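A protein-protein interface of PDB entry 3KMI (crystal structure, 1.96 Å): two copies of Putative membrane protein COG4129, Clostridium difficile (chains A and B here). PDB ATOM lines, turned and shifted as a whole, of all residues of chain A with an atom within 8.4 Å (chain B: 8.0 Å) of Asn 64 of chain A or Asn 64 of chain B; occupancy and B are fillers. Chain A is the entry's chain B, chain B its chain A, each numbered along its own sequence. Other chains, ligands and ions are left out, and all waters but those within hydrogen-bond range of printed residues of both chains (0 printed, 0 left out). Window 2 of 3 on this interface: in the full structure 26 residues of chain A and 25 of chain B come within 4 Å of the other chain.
Among the printed residues, merely in contact across the chains: Asn 64 of chain A with Ile 63 of chain B, Ile 63 of chain A with Ile 63 of chain B and Asp 61 of chain A with Leu 68 of chain B.
Hydrophobic or aromatic side chains of chain B that line the printed part of chain A: Ile 63 and Leu 68.
Among the printed residues, 4 pairs touch across the chains.
Among the printed residues, no Asp or Glu carboxylate lies within 4 Å of a Lys or Arg side-chain nitrogen of the other chain.
The side-chain amide oxygen (OD1) of Asn 64 of chain B lies close to the side-chain amide oxygen (OD1) of Asn 64 of chain A (2.8 Å).
Of the printed residues of chain B, Asp 61 of chain A touches Leu 68.
Ile 63 of chain A touches just one residue of chain B: Ile 63.
Of the printed residues of chain B, Asn 64 of chain A touches Ile 63 (3.5 Å) and Asn 64 (2.8 Å).
Of the printed residues of chain A, Ile 63 of chain B touches Ile 63 (3.6 Å) and Asn 64 (3.5 Å).
Of the printed residues of chain A, Asn 64 of chain B touches Asn 64.
Asn 65 of chain B touches none of the printed residues of chain A.
Leu 67 of chain B touches none of the printed residues of chain A.
Of the printed residues of chain A, Leu 68 of chain B touches Asp 61 (3.7 Å).
The nearest printed residue of chain B that does not touch Asn 64 of chain A is Leu 68 of chain B (4.9 Å).
The nearest printed residue of chain A that does not touch Asn 64 of chain B is Ile 63 of chain A (6.5 Å).
The nearest printed residue of chain B that does not touch Asp 61 of chain A is Thr 71 of chain B (7.9 Å).
Ile 63 of chain A touches its own counterpart, Ile 63 of chain B.
Asn 64 of chain A touches Ile 63 of chain B, but with the chains exchanged Ile 63 of chain A does not touch Asn 64 of chain B (6.5 Å).
Asn 64 of chain B touches its own counterpart, Asn 64 of chain A.
Positions printed for both chains: 59, 60, 61, 62, 63, 64, 65, 66, 67 and 71.
Of the 4 pairs that touch across the chains among the printed residues, 2 have their exchanged pair printed and touching as well.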
ATOM      1  N   GLU A  58     -24.172  -4.730  19.885  1.00  0.00           N
ATOM      2  CA  GLU A  58     -25.088  -3.731  20.437  1.00  0.00           C
ATOM      3  C   GLU A  58     -24.552  -2.299  20.358  1.00  0.00           C
ATOM      4  O   GLU A  58     -25.271  -1.384  19.947  1.00  0.00           O
ATOM      5  CB  GLU A  58     -25.433  -4.086  21.879  1.00  0.00           C
ATOM      6  CG  GLU A  58     -26.576  -5.072  21.967  1.00  0.00           C
ATOM      7  CD  GLU A  58     -26.544  -5.903  23.226  1.00  0.00           C
ATOM      8  OE1 GLU A  58     -25.825  -5.529  24.184  1.00  0.00           O
ATOM      9  OE2 GLU A  58     -27.235  -6.947  23.258  1.00  0.00           O
ATOM     10  N   THR A  59     -23.300  -2.122  20.772  1.00  0.00           N
ATOM     11  CA  THR A  59     -22.602  -0.824  20.730  1.00  0.00           C
ATOM     12  C   THR A  59     -22.685  -0.143  19.361  1.00  0.00           C
ATOM     13  O   THR A  59     -22.950   1.053  19.275  1.00  0.00           O
ATOM     14  CB  THR A  59     -21.124  -0.983  21.180  1.00  0.00           C
ATOM     15  OG1 THR A  59     -21.109  -1.340  22.563  1.00  0.00           O
ATOM     16  CG2 THR A  59     -20.327   0.322  20.990  1.00  0.00           C
ATOM     17  N   TYR A  60     -22.496  -0.929  18.305  1.00  0.00           N
ATOM     18  CA  TYR A  60     -22.625  -0.464  16.922  1.00  0.00           C
ATOM     19  C   TYR A  60     -24.066  -0.242  16.456  1.00  0.00           C
ATOM     20  O   TYR A  60     -24.328   0.661  15.645  1.00  0.00           O
ATOM     21  CB  TYR A  60     -21.935  -1.453  15.995  1.00  0.00           C
ATOM     22  CG  TYR A  60     -20.422  -1.529  16.202  1.00  0.00           C
ATOM     23  CD1 TYR A  60     -19.690  -0.386  16.545  1.00  0.00           C
ATOM     24  CD2 TYR A  60     -19.732  -2.722  16.021  1.00  0.00           C
ATOM     25  CE1 TYR A  60     -18.305  -0.425  16.710  1.00  0.00           C
ATOM     26  CE2 TYR A  60     -18.343  -2.774  16.180  1.00  0.00           C
ATOM     27  CZ  TYR A  60     -17.638  -1.620  16.532  1.00  0.00           C
ATOM     28  OH  TYR A  60     -16.259  -1.635  16.706  1.00  0.00           O
ATOM     29  N   ASP A  61     -24.979  -1.081  16.930  1.00  0.00           N
ATOM     30  CA  ASP A  61     -26.435  -0.899  16.714  1.00  0.00           C
ATOM     31  C   ASP A  61     -26.885   0.476  17.227  1.00  0.00           C
ATOM     32  O   ASP A  61     -27.831   1.088  16.717  1.00  0.00           O
ATOM     33  CB  ASP A  61     -27.216  -1.979  17.488  1.00  0.00           C
ATOM     34  CG  ASP A  61     -27.244  -3.343  16.783  1.00  0.00           C
ATOM     35  OD1 ASP A  61     -26.816  -3.470  15.620  1.00  0.00           O
ATOM     36  OD2 ASP A  61     -27.729  -4.308  17.407  1.00  0.00           O
ATOM     37  N   ASN A  62     -26.179   0.922  18.257  1.00  0.00           N
ATOM     38  CA  ASN A  62     -26.451   2.115  19.030  1.00  0.00           C
ATOM     39  C   ASN A  62     -25.667   3.315  18.516  1.00  0.00           C
ATOM     40  O   ASN A  62     -25.833   4.415  19.032  1.00  0.00           O
ATOM     41  CB  ASN A  62     -26.001   1.830  20.466  1.00  0.00           C
ATOM     42  CG  ASN A  62     -26.782   2.609  21.499  1.00  0.00           C
ATOM     43  OD1 ASN A  62     -26.690   3.832  21.567  1.00  0.00           O
ATOM     44  ND2 ASN A  62     -27.544   1.896  22.331  1.00  0.00           N
ATOM     45  N   ILE A  63     -24.810   3.095  17.516  1.00  0.00           N
ATOM     46  CA  ILE A  63     -23.859   4.110  17.039  1.00  0.00           C
ATOM     47  C   ILE A  63     -24.425   5.523  16.886  1.00  0.00           C
ATOM     48  O   ILE A  63     -23.788   6.470  17.339  1.00  0.00           O
ATOM     49  CB  ILE A  63     -23.179   3.661  15.736  1.00  0.00           C
ATOM     50  N   ASN A  64     -25.610   5.663  16.277  1.00  0.00           N
ATOM     51  CA  ASN A  64     -26.144   6.995  15.896  1.00  0.00           C
ATOM     52  C   ASN A  64     -27.044   7.703  16.930  1.00  0.00           C
ATOM     53  O   ASN A  64     -27.588   8.769  16.649  1.00  0.00           O
ATOM     54  CB  ASN A  64     -26.822   6.941  14.511  1.00  0.00           C
ATOM     55  CG  ASN A  64     -26.827   8.296  13.783  1.00  0.00           C
ATOM     56  OD1 ASN A  64     -25.966   9.149  14.015  1.00  0.00           O
ATOM     57  ND2 ASN A  64     -27.791   8.485  12.880  1.00  0.00           N
ATOM     58  N   ASN A  65     -27.189   7.128  18.122  1.00  0.00           N
ATOM     59  CA  ASN A  65     -27.889   7.816  19.217  1.00  0.00           C
ATOM     60  C   ASN A  65     -27.024   8.174  20.449  1.00  0.00           C
ATOM     61  O   ASN A  65     -27.170   9.274  20.992  1.00  0.00           O
ATOM     62  CB  ASN A  65     -29.221   7.115  19.592  1.00  0.00           C
ATOM     63  CG  ASN A  65     -29.035   5.914  20.508  1.00  0.00           C
ATOM     64  OD1 ASN A  65     -28.547   6.047  21.631  1.00  0.00           O
ATOM     65  ND2 ASN A  65     -29.449   4.733  20.041  1.00  0.00           N
ATOM     66  N   THR A  66     -26.132   7.261  20.864  1.00  0.00           N
ATOM     67  CA  THR A  66     -25.216   7.461  22.017  1.00  0.00           C
ATOM     68  C   THR A  66     -24.019   8.400  21.735  1.00  0.00           C
ATOM     69  O   THR A  66     -23.640   8.606  20.578  1.00  0.00           O
ATOM     70  CB  THR A  66     -24.707   6.103  22.610  1.00  0.00           C
ATOM     71  OG1 THR A  66     -23.698   6.341  23.605  1.00  0.00           O
ATOM     72  CG2 THR A  66     -24.125   5.191  21.531  1.00  0.00           C
ATOM     73  N   LEU A  67     -23.429   8.953  22.800  1.00  0.00           N
ATOM     74  CA  LEU A  67     -22.298   9.889  22.701  1.00  0.00           C
ATOM     75  C   LEU A  67     -21.049   9.264  22.038  1.00  0.00           C
ATOM     76  O   LEU A  67     -20.938   8.042  21.933  1.00  0.00           O
ATOM     77  CB  LEU A  67     -21.965  10.465  24.090  1.00  0.00           C
ATOM     78  CG  LEU A  67     -21.165  11.775  24.203  1.00  0.00           C
ATOM     79  CD1 LEU A  67     -21.957  12.991  23.694  1.00  0.00           C
ATOM     80  CD2 LEU A  67     -20.684  12.018  25.626  1.00  0.00           C
ATOM     81  N   THR A  71     -18.372   6.080  23.589  1.00  0.00           N
ATOM     82  CA  THR A  71     -18.275   4.907  22.705  1.00  0.00           C
ATOM     83  C   THR A  71     -16.808   4.495  22.575  1.00  0.00           C
ATOM     84  O   THR A  71     -16.472   3.322  22.726  1.00  0.00           O
ATOM     85  CB  THR A  71     -18.894   5.155  21.307  1.00  0.00           C
ATOM     86  OG1 THR A  71     -20.312   5.200  21.427  1.00  0.00           O
ATOM     87  CG2 THR A  71     -18.524   4.031  20.324  1.00  0.00           C
ATOM     88  N   THR B  59     -15.279   7.465   9.518  1.00  0.00           N
ATOM     89  CA  THR B  59     -16.524   6.737   9.703  1.00  0.00           C
ATOM     90  C   THR B  59     -17.374   7.410  10.794  1.00  0.00           C
ATOM     91  O   THR B  59     -18.582   7.550  10.631  1.00  0.00           O
ATOM     92  CB  THR B  59     -16.262   5.251  10.021  1.00  0.00           C
ATOM     93  OG1 THR B  59     -15.494   4.673   8.950  1.00  0.00           O
ATOM     94  CG2 THR B  59     -17.615   4.459  10.201  1.00  0.00           C
ATOM     95  N   TYR B  60     -16.728   7.854  11.877  1.00  0.00           N
ATOM     96  CA  TYR B  60     -17.414   8.468  13.017  1.00  0.00           C
ATOM     97  C   TYR B  60     -18.004   9.803  12.619  1.00  0.00           C
ATOM     98  O   TYR B  60     -19.095  10.161  13.048  1.00  0.00           O
ATOM     99  CB  TYR B  60     -16.446   8.728  14.175  1.00  0.00           C
ATOM    100  CG  TYR B  60     -16.046   7.531  15.008  1.00  0.00           C
ATOM    101  CD1 TYR B  60     -16.776   6.330  14.974  1.00  0.00           C
ATOM    102  CD2 TYR B  60     -14.952   7.619  15.871  1.00  0.00           C
ATOM    103  CE1 TYR B  60     -16.398   5.233  15.756  1.00  0.00           C
ATOM    104  CE2 TYR B  60     -14.579   6.542  16.662  1.00  0.00           C
ATOM    105  CZ  TYR B  60     -15.304   5.350  16.602  1.00  0.00           C
ATOM    106  OH  TYR B  60     -14.905   4.280  17.386  1.00  0.00           O
ATOM    107  N   ASP B  61     -17.241  10.544  11.822  1.00  0.00           N
ATOM    108  CA  ASP B  61     -17.657  11.834  11.301  1.00  0.00           C
ATOM    109  C   ASP B  61     -19.006  11.736  10.577  1.00  0.00           C
ATOM    110  O   ASP B  61     -19.808  12.689  10.624  1.00  0.00           O
ATOM    111  CB  ASP B  61     -16.609  12.381  10.337  1.00  0.00           C
ATOM    112  CG  ASP B  61     -15.454  13.113  11.051  1.00  0.00           C
ATOM    113  OD1 ASP B  61     -15.523  13.347  12.279  1.00  0.00           O
ATOM    114  OD2 ASP B  61     -14.470  13.461  10.365  1.00  0.00           O
ATOM    115  N   ASN B  62     -19.251  10.582   9.952  1.00  0.00           N
ATOM    116  CA  ASN B  62     -20.360  10.400   9.000  1.00  0.00           C
ATOM    117  C   ASN B  62     -21.442   9.473   9.494  1.00  0.00           C
ATOM    118  O   ASN B  62     -22.288   9.036   8.707  1.00  0.00           O
ATOM    119  CB  ASN B  62     -19.850   9.811   7.688  1.00  0.00           C
ATOM    120  CG  ASN B  62     -19.292  10.850   6.756  1.00  0.00           C
ATOM    121  OD1 ASN B  62     -20.032  11.548   6.087  1.00  0.00           O
ATOM    122  ND2 ASN B  62     -17.974  10.918   6.665  1.00  0.00           N
ATOM    123  N   ILE B  63     -21.442   9.160  10.783  1.00  0.00           N
ATOM    124  CA  ILE B  63     -22.521   8.330  11.323  1.00  0.00           C
ATOM    125  C   ILE B  63     -23.888   8.993  11.091  1.00  0.00           C
ATOM    126  O   ILE B  63     -24.872   8.302  10.788  1.00  0.00           O
ATOM    127  CB  ILE B  63     -22.300   7.903  12.815  1.00  0.00           C
ATOM    128  CG1 ILE B  63     -22.148   9.120  13.748  1.00  0.00           C
ATOM    129  CG2 ILE B  63     -21.109   6.970  12.916  1.00  0.00           C
ATOM    130  CD1 ILE B  63     -21.939   8.780  15.252  1.00  0.00           C
ATOM    131  N   ASN B  64     -23.941  10.320  11.207  1.00  0.00           N
ATOM    132  CA  ASN B  64     -25.186  11.065  11.031  1.00  0.00           C
ATOM    133  C   ASN B  64     -25.783  10.980   9.624  1.00  0.00           C
ATOM    134  O   ASN B  64     -26.992  11.117   9.464  1.00  0.00           O
ATOM    135  CB  ASN B  64     -24.992  12.526  11.438  1.00  0.00           C
ATOM    136  CG  ASN B  64     -24.770  12.687  12.928  1.00  0.00           C
ATOM    137  OD1 ASN B  64     -24.843  11.716  13.684  1.00  0.00           O
ATOM    138  ND2 ASN B  64     -24.510  13.917  13.362  1.00  0.00           N
ATOM    139  N   ASN B  65     -24.935  10.742   8.624  1.00  0.00           N
ATOM    140  CA  ASN B  65     -25.349  10.714   7.223  1.00  0.00           C
ATOM    141  C   ASN B  65     -25.149   9.374   6.511  1.00  0.00           C
ATOM    142  O   ASN B  65     -25.302   9.286   5.290  1.00  0.00           O
ATOM    143  CB  ASN B  65     -24.617  11.805   6.432  1.00  0.00           C
ATOM    144  CG  ASN B  65     -25.052  13.221   6.817  1.00  0.00           C
ATOM    145  OD1 ASN B  65     -26.244  13.568   6.771  1.00  0.00           O
ATOM    146  ND2 ASN B  65     -24.073  14.058   7.172  1.00  0.00           N
ATOM    147  N   THR B  66     -24.817   8.325   7.257  1.00  0.00           N
ATOM    148  CA  THR B  66     -24.567   7.030   6.625  1.00  0.00           C
ATOM    149  C   THR B  66     -25.621   5.997   6.953  1.00  0.00           C
ATOM    150  O   THR B  66     -26.157   5.957   8.075  1.00  0.00           O
ATOM    151  CB  THR B  66     -23.163   6.482   6.966  1.00  0.00           C
ATOM    152  OG1 THR B  66     -22.180   7.438   6.562  1.00  0.00           O
ATOM    153  CG2 THR B  66     -22.889   5.157   6.229  1.00  0.00           C
ATOM    154  N   LEU B  67     -25.930   5.174   5.950  1.00  0.00           N
ATOM    155  CA  LEU B  67     -26.711   3.986   6.162  1.00  0.00           C
ATOM    156  C   LEU B  67     -25.986   3.243   7.270  1.00  0.00           C
ATOM    157  O   LEU B  67     -24.841   2.798   7.077  1.00  0.00           O
ATOM    158  CB  LEU B  67     -26.725   3.133   4.890  1.00  0.00           C
ATOM    159  CG  LEU B  67     -28.082   2.678   4.339  1.00  0.00           C
ATOM    160  CD1 LEU B  67     -28.951   3.886   3.940  1.00  0.00           C
ATOM    161  CD2 LEU B  67     -27.867   1.742   3.161  1.00  0.00           C
ATOM    162  N   LEU B  68     -26.637   3.121   8.425  1.00  0.00           N
ATOM    163  CA  LEU B  68     -26.061   2.392   9.548  1.00  0.00           C
ATOM    164  C   LEU B  68     -25.602   0.988   9.109  1.00  0.00           C
ATOM    165  O   LEU B  68     -24.761   0.368   9.757  1.00  0.00           O
ATOM    166  CB  LEU B  68     -27.051   2.321  10.713  1.00  0.00           C
ATOM    167  CG  LEU B  68     -26.521   1.675  11.991  1.00  0.00           C
ATOM    168  CD1 LEU B  68     -27.261   2.213  13.192  1.00  0.00           C
ATOM    169  CD2 LEU B  68     -26.634   0.165  11.910  1.00  0.00           C
ATOM    170  N   THR B  71     -22.046   1.544   7.898  1.00  0.00           N
ATOM    171  CA  THR B  71     -21.277   1.932   9.096  1.00  0.00           C
ATOM    172  C   THR B  71     -20.917   0.685   9.900  1.00  0.00           C
ATOM    173  O   THR B  71     -19.800   0.575  10.440  1.00  0.00           O
ATOM    174  CB  THR B  71     -22.062   2.938  10.001  1.00  0.00           C
ATOM    175  OG1 THR B  71     -22.194   4.213   9.345  1.00  0.00           O
ATOM    176  CG2 THR B  71     -21.366   3.152  11.342  1.00  0.00           C
